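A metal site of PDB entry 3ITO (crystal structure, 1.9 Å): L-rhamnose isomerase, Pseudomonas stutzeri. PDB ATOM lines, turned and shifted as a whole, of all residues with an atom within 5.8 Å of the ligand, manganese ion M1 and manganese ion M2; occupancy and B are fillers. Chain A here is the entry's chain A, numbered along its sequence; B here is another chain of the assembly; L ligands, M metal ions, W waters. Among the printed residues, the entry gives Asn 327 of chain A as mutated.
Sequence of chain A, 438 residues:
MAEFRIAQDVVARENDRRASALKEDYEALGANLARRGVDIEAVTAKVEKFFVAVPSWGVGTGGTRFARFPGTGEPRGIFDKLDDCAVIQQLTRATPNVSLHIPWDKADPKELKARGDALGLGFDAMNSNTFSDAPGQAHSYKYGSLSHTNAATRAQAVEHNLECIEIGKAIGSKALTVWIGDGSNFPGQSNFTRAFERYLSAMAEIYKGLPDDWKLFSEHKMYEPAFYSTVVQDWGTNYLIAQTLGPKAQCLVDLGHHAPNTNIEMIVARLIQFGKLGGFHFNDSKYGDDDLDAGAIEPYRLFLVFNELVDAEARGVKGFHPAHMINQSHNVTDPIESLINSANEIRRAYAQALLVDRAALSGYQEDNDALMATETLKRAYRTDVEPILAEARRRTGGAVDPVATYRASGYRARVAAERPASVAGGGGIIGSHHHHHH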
ATOM      1  N   TRP A  57      21.980  10.377  17.376  1.00  0.00           N
ATOM      2  CA  TRP A  57      21.637   9.719  18.631  1.00  0.00           C
ATOM      3  C   TRP A  57      22.161   8.286  18.752  1.00  0.00           C
ATOM      4  O   TRP A  57      21.988   7.634  19.776  1.00  0.00           O
ATOM      5  CB  TRP A  57      20.117   9.749  18.847  1.00  0.00           C
ATOM      6  CG  TRP A  57      19.317   9.005  17.811  1.00  0.00           C
ATOM      7  CD1 TRP A  57      18.846   7.718  17.905  1.00  0.00           C
ATOM      8  CD2 TRP A  57      18.883   9.498  16.541  1.00  0.00           C
ATOM      9  NE1 TRP A  57      18.148   7.384  16.768  1.00  0.00           N
ATOM     10  CE2 TRP A  57      18.162   8.460  15.914  1.00  0.00           C
ATOM     11  CE3 TRP A  57      19.045  10.708  15.860  1.00  0.00           C
ATOM     12  CZ2 TRP A  57      17.598   8.600  14.633  1.00  0.00           C
ATOM     13  CZ3 TRP A  57      18.481  10.852  14.599  1.00  0.00           C
ATOM     14  CH2 TRP A  57      17.770   9.799  13.995  1.00  0.00           C
ATOM     15  N   HIS A 101      18.159  14.862  15.331  1.00  0.00           N
ATOM     16  CA  HIS A 101      16.898  14.661  16.029  1.00  0.00           C
ATOM     17  C   HIS A 101      16.647  15.890  16.896  1.00  0.00           C
ATOM     18  O   HIS A 101      17.474  16.275  17.723  1.00  0.00           O
ATOM     19  CB  HIS A 101      16.958  13.398  16.896  1.00  0.00           C
ATOM     20  CG  HIS A 101      15.713  12.572  16.847  1.00  0.00           C
ATOM     21  ND1 HIS A 101      14.478  13.067  17.231  1.00  0.00           N
ATOM     22  CD2 HIS A 101      15.495  11.301  16.421  1.00  0.00           C
ATOM     23  CE1 HIS A 101      13.553  12.134  17.049  1.00  0.00           C
ATOM     24  NE2 HIS A 101      14.146  11.052  16.561  1.00  0.00           N
ATOM     25  N   TRP A 104      16.575  17.086  20.704  1.00  0.00           N
ATOM     26  CA  TRP A 104      17.841  16.588  21.246  1.00  0.00           C
ATOM     27  C   TRP A 104      19.064  17.335  20.711  1.00  0.00           C
ATOM     28  O   TRP A 104      19.981  17.669  21.453  1.00  0.00           O
ATOM     29  CB  TRP A 104      18.043  15.100  20.950  1.00  0.00           C
ATOM     30  CG  TRP A 104      17.035  14.187  21.561  1.00  0.00           C
ATOM     31  CD1 TRP A 104      16.239  14.448  22.636  1.00  0.00           C
ATOM     32  CD2 TRP A 104      16.735  12.857  21.149  1.00  0.00           C
ATOM     33  NE1 TRP A 104      15.463  13.351  22.918  1.00  0.00           N
ATOM     34  CE2 TRP A 104      15.735  12.361  22.017  1.00  0.00           C
ATOM     35  CE3 TRP A 104      17.207  12.028  20.119  1.00  0.00           C
ATOM     36  CZ2 TRP A 104      15.206  11.076  21.899  1.00  0.00           C
ATOM     37  CZ3 TRP A 104      16.687  10.747  20.000  1.00  0.00           C
ATOM     38  CH2 TRP A 104      15.684  10.286  20.882  1.00  0.00           C
ATOM     39  N   ASN A 127      14.696  14.775  11.924  1.00  0.00           N
ATOM     40  CA  ASN A 127      13.776  13.884  12.620  1.00  0.00           C
ATOM     41  C   ASN A 127      13.085  14.678  13.714  1.00  0.00           C
ATOM     42  O   ASN A 127      13.750  15.261  14.571  1.00  0.00           O
ATOM     43  CB  ASN A 127      14.518  12.706  13.235  1.00  0.00           C
ATOM     44  CG  ASN A 127      15.121  11.779  12.189  1.00  0.00           C
ATOM     45  OD1 ASN A 127      14.479  10.830  11.737  1.00  0.00           O
ATOM     46  ND2 ASN A 127      16.356  12.063  11.781  1.00  0.00           N
ATOM     47  N   SER A 128      11.751  14.698  13.692  1.00  0.00           N
ATOM     48  CA  SER A 128      10.988  15.412  14.712  1.00  0.00           C
ATOM     49  C   SER A 128      10.743  14.501  15.919  1.00  0.00           C
ATOM     50  O   SER A 128      10.847  13.279  15.810  1.00  0.00           O
ATOM     51  CB  SER A 128       9.649  15.894  14.144  1.00  0.00           C
ATOM     52  OG  SER A 128       8.881  14.805  13.671  1.00  0.00           O
ATOM     53  N   PHE A 131       7.143  12.357  20.682  1.00  0.00           N
ATOM     54  CA  PHE A 131       6.891  11.111  21.393  1.00  0.00           C
ATOM     55  C   PHE A 131       7.427  11.218  22.821  1.00  0.00           C
ATOM     56  O   PHE A 131       7.464  10.250  23.583  1.00  0.00           O
ATOM     57  CB  PHE A 131       7.518   9.912  20.651  1.00  0.00           C
ATOM     58  CG  PHE A 131       8.993  10.059  20.353  1.00  0.00           C
ATOM     59  CD1 PHE A 131       9.951   9.874  21.345  1.00  0.00           C
ATOM     60  CD2 PHE A 131       9.424  10.359  19.051  1.00  0.00           C
ATOM     61  CE1 PHE A 131      11.304   9.977  21.059  1.00  0.00           C
ATOM     62  CE2 PHE A 131      10.776  10.460  18.755  1.00  0.00           C
ATOM     63  CZ  PHE A 131      11.726  10.273  19.758  1.00  0.00           C
ATOM     64  N   THR A 177      11.597  13.451   8.586  1.00  0.00           N
ATOM     65  CA  THR A 177      11.068  12.133   8.922  1.00  0.00           C
ATOM     66  C   THR A 177      10.177  12.275  10.146  1.00  0.00           C
ATOM     67  O   THR A 177      10.586  12.833  11.168  1.00  0.00           O
ATOM     68  CB  THR A 177      12.177  11.142   9.237  1.00  0.00           C
ATOM     69  OG1 THR A 177      12.906  10.850   8.036  1.00  0.00           O
ATOM     70  CG2 THR A 177      11.598   9.855   9.823  1.00  0.00           C
ATOM     71  N   TRP A 179       8.073  10.177  12.877  1.00  0.00           N
ATOM     72  CA  TRP A 179       7.686   8.950  13.548  1.00  0.00           C
ATOM     73  C   TRP A 179       7.100   9.398  14.877  1.00  0.00           C
ATOM     74  O   TRP A 179       7.729  10.174  15.597  1.00  0.00           O
ATOM     75  CB  TRP A 179       8.869   8.035  13.845  1.00  0.00           C
ATOM     76  CG  TRP A 179       8.427   6.885  14.717  1.00  0.00           C
ATOM     77  CD1 TRP A 179       7.649   5.818  14.342  1.00  0.00           C
ATOM     78  CD2 TRP A 179       8.632   6.745  16.132  1.00  0.00           C
ATOM     79  NE1 TRP A 179       7.370   5.028  15.436  1.00  0.00           N
ATOM     80  CE2 TRP A 179       7.963   5.565  16.548  1.00  0.00           C
ATOM     81  CE3 TRP A 179       9.332   7.495  17.088  1.00  0.00           C
ATOM     82  CZ2 TRP A 179       7.962   5.126  17.883  1.00  0.00           C
ATOM     83  CZ3 TRP A 179       9.331   7.056  18.423  1.00  0.00           C
ATOM     84  CH2 TRP A 179       8.653   5.887  18.797  1.00  0.00           C
ATOM     85  N   GLU A 219       6.796   7.281   9.024  1.00  0.00           N
ATOM     86  CA  GLU A 219       7.326   5.973   9.396  1.00  0.00           C
ATOM     87  C   GLU A 219       6.339   5.135  10.196  1.00  0.00           C
ATOM     88  O   GLU A 219       5.889   5.556  11.261  1.00  0.00           O
ATOM     89  CB  GLU A 219       8.616   6.179  10.202  1.00  0.00           C
ATOM     90  CG  GLU A 219       9.185   4.924  10.837  1.00  0.00           C
ATOM     91  CD  GLU A 219      10.511   5.194  11.528  1.00  0.00           C
ATOM     92  OE1 GLU A 219      10.872   6.379  11.711  1.00  0.00           O
ATOM     93  OE2 GLU A 219      11.200   4.217  11.894  1.00  0.00           O
ATOM     94  N   LYS A 221       5.069   1.748  12.390  1.00  0.00           N
ATOM     95  CA  LYS A 221       5.613   0.874  13.423  1.00  0.00           C
ATOM     96  C   LYS A 221       4.436   0.114  14.021  1.00  0.00           C
ATOM     97  O   LYS A 221       3.443   0.713  14.418  1.00  0.00           O
ATOM     98  CB  LYS A 221       6.332   1.687  14.499  1.00  0.00           C
ATOM     99  CG  LYS A 221       7.143   0.813  15.452  1.00  0.00           C
ATOM    100  CD  LYS A 221       7.907   1.657  16.460  1.00  0.00           C
ATOM    101  CE  LYS A 221       8.651   0.792  17.455  1.00  0.00           C
ATOM    102  NZ  LYS A 221       9.325   1.604  18.512  1.00  0.00           N
ATOM    103  N   GLU A 224       4.847  -0.189  20.193  1.00  0.00           N
ATOM    104  CA  GLU A 224       5.880   0.449  21.018  1.00  0.00           C
ATOM    105  C   GLU A 224       6.096   1.885  20.537  1.00  0.00           C
ATOM    106  O   GLU A 224       6.628   2.113  19.449  1.00  0.00           O
ATOM    107  CB  GLU A 224       7.213  -0.297  20.983  1.00  0.00           C
ATOM    108  CG  GLU A 224       8.231   0.334  21.942  1.00  0.00           C
ATOM    109  CD  GLU A 224       9.641  -0.193  21.803  1.00  0.00           C
ATOM    110  OE1 GLU A 224      10.072  -0.469  20.660  1.00  0.00           O
ATOM    111  OE2 GLU A 224      10.338  -0.304  22.830  1.00  0.00           O
ATOM    112  N   ASP A 254      11.363   0.923   8.375  1.00  0.00           N
ATOM    113  CA  ASP A 254      12.352   0.601   9.392  1.00  0.00           C
ATOM    114  C   ASP A 254      12.238  -0.917   9.579  1.00  0.00           C
ATOM    115  O   ASP A 254      11.205  -1.430   9.993  1.00  0.00           O
ATOM    116  CB  ASP A 254      12.049   1.325  10.711  1.00  0.00           C
ATOM    117  CG  ASP A 254      13.123   1.094  11.769  1.00  0.00           C
ATOM    118  OD1 ASP A 254      13.617   2.085  12.350  1.00  0.00           O
ATOM    119  OD2 ASP A 254      13.454  -0.070  12.028  1.00  0.00           O
ATOM    120  N   HIS A 257      10.309  -2.746  12.489  1.00  0.00           N
ATOM    121  CA  HIS A 257       8.960  -2.302  12.825  1.00  0.00           C
ATOM    122  C   HIS A 257       7.814  -3.136  12.265  1.00  0.00           C
ATOM    123  O   HIS A 257       6.693  -2.649  12.168  1.00  0.00           O
ATOM    124  CB  HIS A 257       8.765  -0.853  12.365  1.00  0.00           C
ATOM    125  CG  HIS A 257       9.616   0.140  13.088  1.00  0.00           C
ATOM    126  ND1 HIS A 257       9.426   1.495  12.971  1.00  0.00           N
ATOM    127  CD2 HIS A 257      10.639  -0.023  13.961  1.00  0.00           C
ATOM    128  CE1 HIS A 257      10.288   2.134  13.750  1.00  0.00           C
ATOM    129  NE2 HIS A 257      11.039   1.227  14.355  1.00  0.00           N
ATOM    130  N   HIS A 281      15.425   2.653   7.330  1.00  0.00           N
ATOM    131  CA  HIS A 281      16.030   2.771   8.633  1.00  0.00           C
ATOM    132  C   HIS A 281      16.574   1.357   8.810  1.00  0.00           C
ATOM    133  O   HIS A 281      15.808   0.398   8.954  1.00  0.00           O
ATOM    134  CB  HIS A 281      15.004   3.106   9.722  1.00  0.00           C
ATOM    135  CG  HIS A 281      14.882   4.582   9.998  1.00  0.00           C
ATOM    136  ND1 HIS A 281      14.238   5.077  11.106  1.00  0.00           N
ATOM    137  CD2 HIS A 281      15.325   5.653   9.304  1.00  0.00           C
ATOM    138  CE1 HIS A 281      14.287   6.395  11.101  1.00  0.00           C
ATOM    139  NE2 HIS A 281      14.940   6.769  10.012  1.00  0.00           N
ATOM    140  N   ASN A 283      18.778  -1.711  10.559  1.00  0.00           N
ATOM    141  CA  ASN A 283      19.102  -2.297  11.850  1.00  0.00           C
ATOM    142  C   ASN A 283      18.718  -3.762  11.721  1.00  0.00           C
ATOM    143  O   ASN A 283      18.251  -4.197  10.667  1.00  0.00           O
ATOM    144  CB  ASN A 283      18.287  -1.613  12.969  1.00  0.00           C
ATOM    145  CG  ASN A 283      16.809  -1.543  12.657  1.00  0.00           C
ATOM    146  OD1 ASN A 283      16.161  -2.568  12.422  1.00  0.00           O
ATOM    147  ND2 ASN A 283      16.257  -0.340  12.641  1.00  0.00           N
ATOM    148  N   ASP A 289      11.383  -4.533  17.983  1.00  0.00           N
ATOM    149  CA  ASP A 289      12.183  -3.442  17.406  1.00  0.00           C
ATOM    150  C   ASP A 289      13.484  -3.431  18.218  1.00  0.00           C
ATOM    151  O   ASP A 289      13.770  -2.480  18.936  1.00  0.00           O
ATOM    152  CB  ASP A 289      11.430  -2.115  17.557  1.00  0.00           C
ATOM    153  CG  ASP A 289      12.165  -0.941  16.926  1.00  0.00           C
ATOM    154  OD1 ASP A 289      12.994  -1.159  16.014  1.00  0.00           O
ATOM    155  OD2 ASP A 289      11.895   0.211  17.339  1.00  0.00           O
ATOM    156  N   ASP A 291      16.581  -3.029  17.403  1.00  0.00           N
ATOM    157  CA  ASP A 291      17.576  -2.021  17.049  1.00  0.00           C
ATOM    158  C   ASP A 291      19.019  -2.515  17.137  1.00  0.00           C
ATOM    159  O   ASP A 291      19.912  -1.787  17.572  1.00  0.00           O
ATOM    160  CB  ASP A 291      17.402  -0.785  17.942  1.00  0.00           C
ATOM    161  CG  ASP A 291      16.156  -0.005  17.621  1.00  0.00           C
ATOM    162  OD1 ASP A 291      15.796   0.022  16.426  1.00  0.00           O
ATOM    163  OD2 ASP A 291      15.542   0.591  18.526  1.00  0.00           O
ATOM    164  N   MET A 325      19.318   5.430   6.012  1.00  0.00           N
ATOM    165  CA  MET A 325      19.825   5.796   7.332  1.00  0.00           C
ATOM    166  C   MET A 325      19.872   4.607   8.277  1.00  0.00           C
ATOM    167  O   MET A 325      19.035   3.699   8.200  1.00  0.00           O
ATOM    168  CB  MET A 325      18.959   6.887   7.969  1.00  0.00           C
ATOM    169  CG  MET A 325      19.520   7.381   9.304  1.00  0.00           C
ATOM    170  SD  MET A 325      18.391   8.407  10.277  1.00  0.00           S
ATOM    171  CE  MET A 325      17.763   7.189  11.462  1.00  0.00           C
ATOM    172  N   ASN A 327      19.417   3.256  11.966  1.00  0.00           N
ATOM    173  CA  ASN A 327      18.665   3.669  13.155  1.00  0.00           C
ATOM    174  C   ASN A 327      18.802   2.505  14.123  1.00  0.00           C
ATOM    175  O   ASN A 327      18.036   1.545  14.073  1.00  0.00           O
ATOM    176  CB  ASN A 327      17.188   3.906  12.831  1.00  0.00           C
ATOM    177  CG  ASN A 327      16.423   4.448  14.026  1.00  0.00           C
ATOM    178  OD1 ASN A 327      16.907   5.325  14.752  1.00  0.00           O
ATOM    179  ND2 ASN A 327      15.223   3.935  14.242  1.00  0.00           N
ATOM    180  N   ARG B  65      11.078   2.993  26.828  1.00  0.00           N
ATOM    181  CA  ARG B  65      12.417   3.515  26.616  1.00  0.00           C
ATOM    182  C   ARG B  65      12.377   4.869  25.895  1.00  0.00           C
ATOM    183  O   ARG B  65      13.394   5.551  25.795  1.00  0.00           O
ATOM    184  CB  ARG B  65      13.260   2.527  25.798  1.00  0.00           C
ATOM    185  CG  ARG B  65      12.664   2.184  24.456  1.00  0.00           C
ATOM    186  CD  ARG B  65      13.629   1.380  23.600  1.00  0.00           C
ATOM    187  NE  ARG B  65      12.958   0.870  22.404  1.00  0.00           N
ATOM    188  CZ  ARG B  65      13.573   0.581  21.268  1.00  0.00           C
ATOM    189  NH1 ARG B  65      14.874   0.744  21.145  1.00  0.00           N
ATOM    190  NH2 ARG B  65      12.859   0.135  20.234  1.00  0.00           N
ATOM    191  N   PHE B  66      11.211   5.253  25.391  1.00  0.00           N
ATOM    192  CA  PHE B  66      11.047   6.517  24.680  1.00  0.00           C
ATOM    193  C   PHE B  66      10.592   7.667  25.578  1.00  0.00           C
ATOM    194  O   PHE B  66      10.983   8.808  25.371  1.00  0.00           O
ATOM    195  CB  PHE B  66      10.037   6.361  23.540  1.00  0.00           C
ATOM    196  CG  PHE B  66      10.491   5.416  22.472  1.00  0.00           C
ATOM    197  CD1 PHE B  66      11.454   5.808  21.553  1.00  0.00           C
ATOM    198  CD2 PHE B  66       9.994   4.124  22.415  1.00  0.00           C
ATOM    199  CE1 PHE B  66      11.925   4.922  20.585  1.00  0.00           C
ATOM    200  CE2 PHE B  66      10.452   3.222  21.460  1.00  0.00           C
ATOM    201  CZ  PHE B  66      11.424   3.620  20.550  1.00  0.00           C
HETATM  202  C1  LIG L   1      11.040   4.450  16.640  1.00  0.00           C
HETATM  203  O1  LIG L   1      11.341   3.223  17.258  1.00  0.00           O
HETATM  204  C2  LIG L   1      12.181   4.920  15.752  1.00  0.00           C
HETATM  205  O2  LIG L   1      12.435   3.987  14.718  1.00  0.00           O
HETATM  206  C3  LIG L   1      11.927   6.321  15.170  1.00  0.00           C
HETATM  207  O3  LIG L   1      12.534   6.404  13.883  1.00  0.00           O
HETATM  208  C4  LIG L   1      12.648   7.251  16.143  1.00  0.00           C
HETATM  209  O4  LIG L   1      13.148   8.393  15.454  1.00  0.00           O
HETATM  210  C5  LIG L   1      13.798   6.391  16.655  1.00  0.00           C
HETATM  211  O5  LIG L   1      13.361   5.032  16.569  1.00  0.00           O
HETATM  212  C6  LIG L   1      14.166   6.657  18.100  1.00  0.00           C
HETATM  213  O6  LIG L   1      15.505   6.266  18.355  1.00  0.00           O
HETATM  214 MN    MN M   1      13.137   4.200  12.762  1.00  0.00          MN
HETATM  215 MN    MN M   2      12.422   1.813  15.809  1.00  0.00          MN
HETATM  216  O   HOH W   1      13.943   2.469  17.490  1.00  0.00           O
HETATM  217  O   HOH W   2      12.382   9.613  13.274  1.00  0.00           O
HETATM  218  O   HOH W   3      14.109   1.027  14.977  1.00  0.00           O
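NZ of Lys 221 sits close to O1 of the ligand (2.9 Å).
NE1 of Trp 57 sits at hydrogen-bond distance from O6 of the ligand (3.3 Å).
NE2 of His 101 sits at hydrogen-bond distance from O4 of the ligand.
NZ of Lys 221 sits close to OD2 of Asp 289 (3.1 Å).
NE1 of Trp 57 is in hydrogen-bond range of OD1 of Asn 327, at 3.1 Å.
The side-chain carboxylate (OD2) of Asp 291 is in salt-bridge range of the guanidinium group (NH1) of Arg 65 of chain B (2.7 Å).
OD2 of Asp 254 sits at hydrogen-bond distance from ND2 of Asn 283 (2.9 Å).
The backbone carbonyl oxygen (O) of Asp 289 sits at hydrogen-bond distance from the guanidinium group (NH2) of Arg 65 of chain B, 3.1 Å away.
The side-chain amide nitrogen (ND2) of Asn 283 lies within hydrogen-bond range of the backbone carbonyl oxygen (O) of Asn 327 (3.0 Å).
ND1 of His 257 lies close to OE2 of Glu 219 (3.4 Å).
NZ of Lys 221 lies within salt-bridge range of OE1 of Glu 224.
Residues that only touch the ligand: Trp 179 and Phe 66 of chain B.
The nearest printed residue that does not touch the ligand is Phe 131 (4.5 Å).
Five residues have an atom within 4 Å of manganese ion M1: Glu 219, Asp 254, His 257, His 281 and Asn 327.
Residues that only touch manganese ion M2: Asp 291.
Five residues have an atom within 4 Å of manganese ion M2: Asp 254, His 257, Asp 289, Asp 291 and Asn 327.
The nearest printed residue that does not touch manganese ion M2 is Lys 221 (4.1 Å).
Manganese ion M1 is bound by an oxygen (O2) of the ligand, the side-chain carboxylate (OE2) of Glu 219, a ring nitrogen (ND1) of His 281, the side-chain carboxylate (OD1) of Asp 254, an oxygen (O3) of the ligand and the side-chain amide nitrogen (ND2) of Asn 327.
Manganese ion M2 is bound by water W3, at 2.0 Å.
Manganese ion M2 is bound by NE2 of His 257 (2.1 Å).
The side-chain carboxylate (OD2) of Asp 289 is bound to manganese ion M2, 2.3 Å away.
O1 of the ligand is bound to manganese ion M2.
Water W1 binds manganese ion M2 (2.4 Å).
O2 of the ligand binds manganese ion M2 (2.4 Å).
Water W1 bridges OD2 of Asp 291 (2.7 Å) and O5 of the ligand (2.8 Å).
Water W2 bridges an oxygen (O4) of the ligand and the side-chain amide oxygen of Asn 127.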
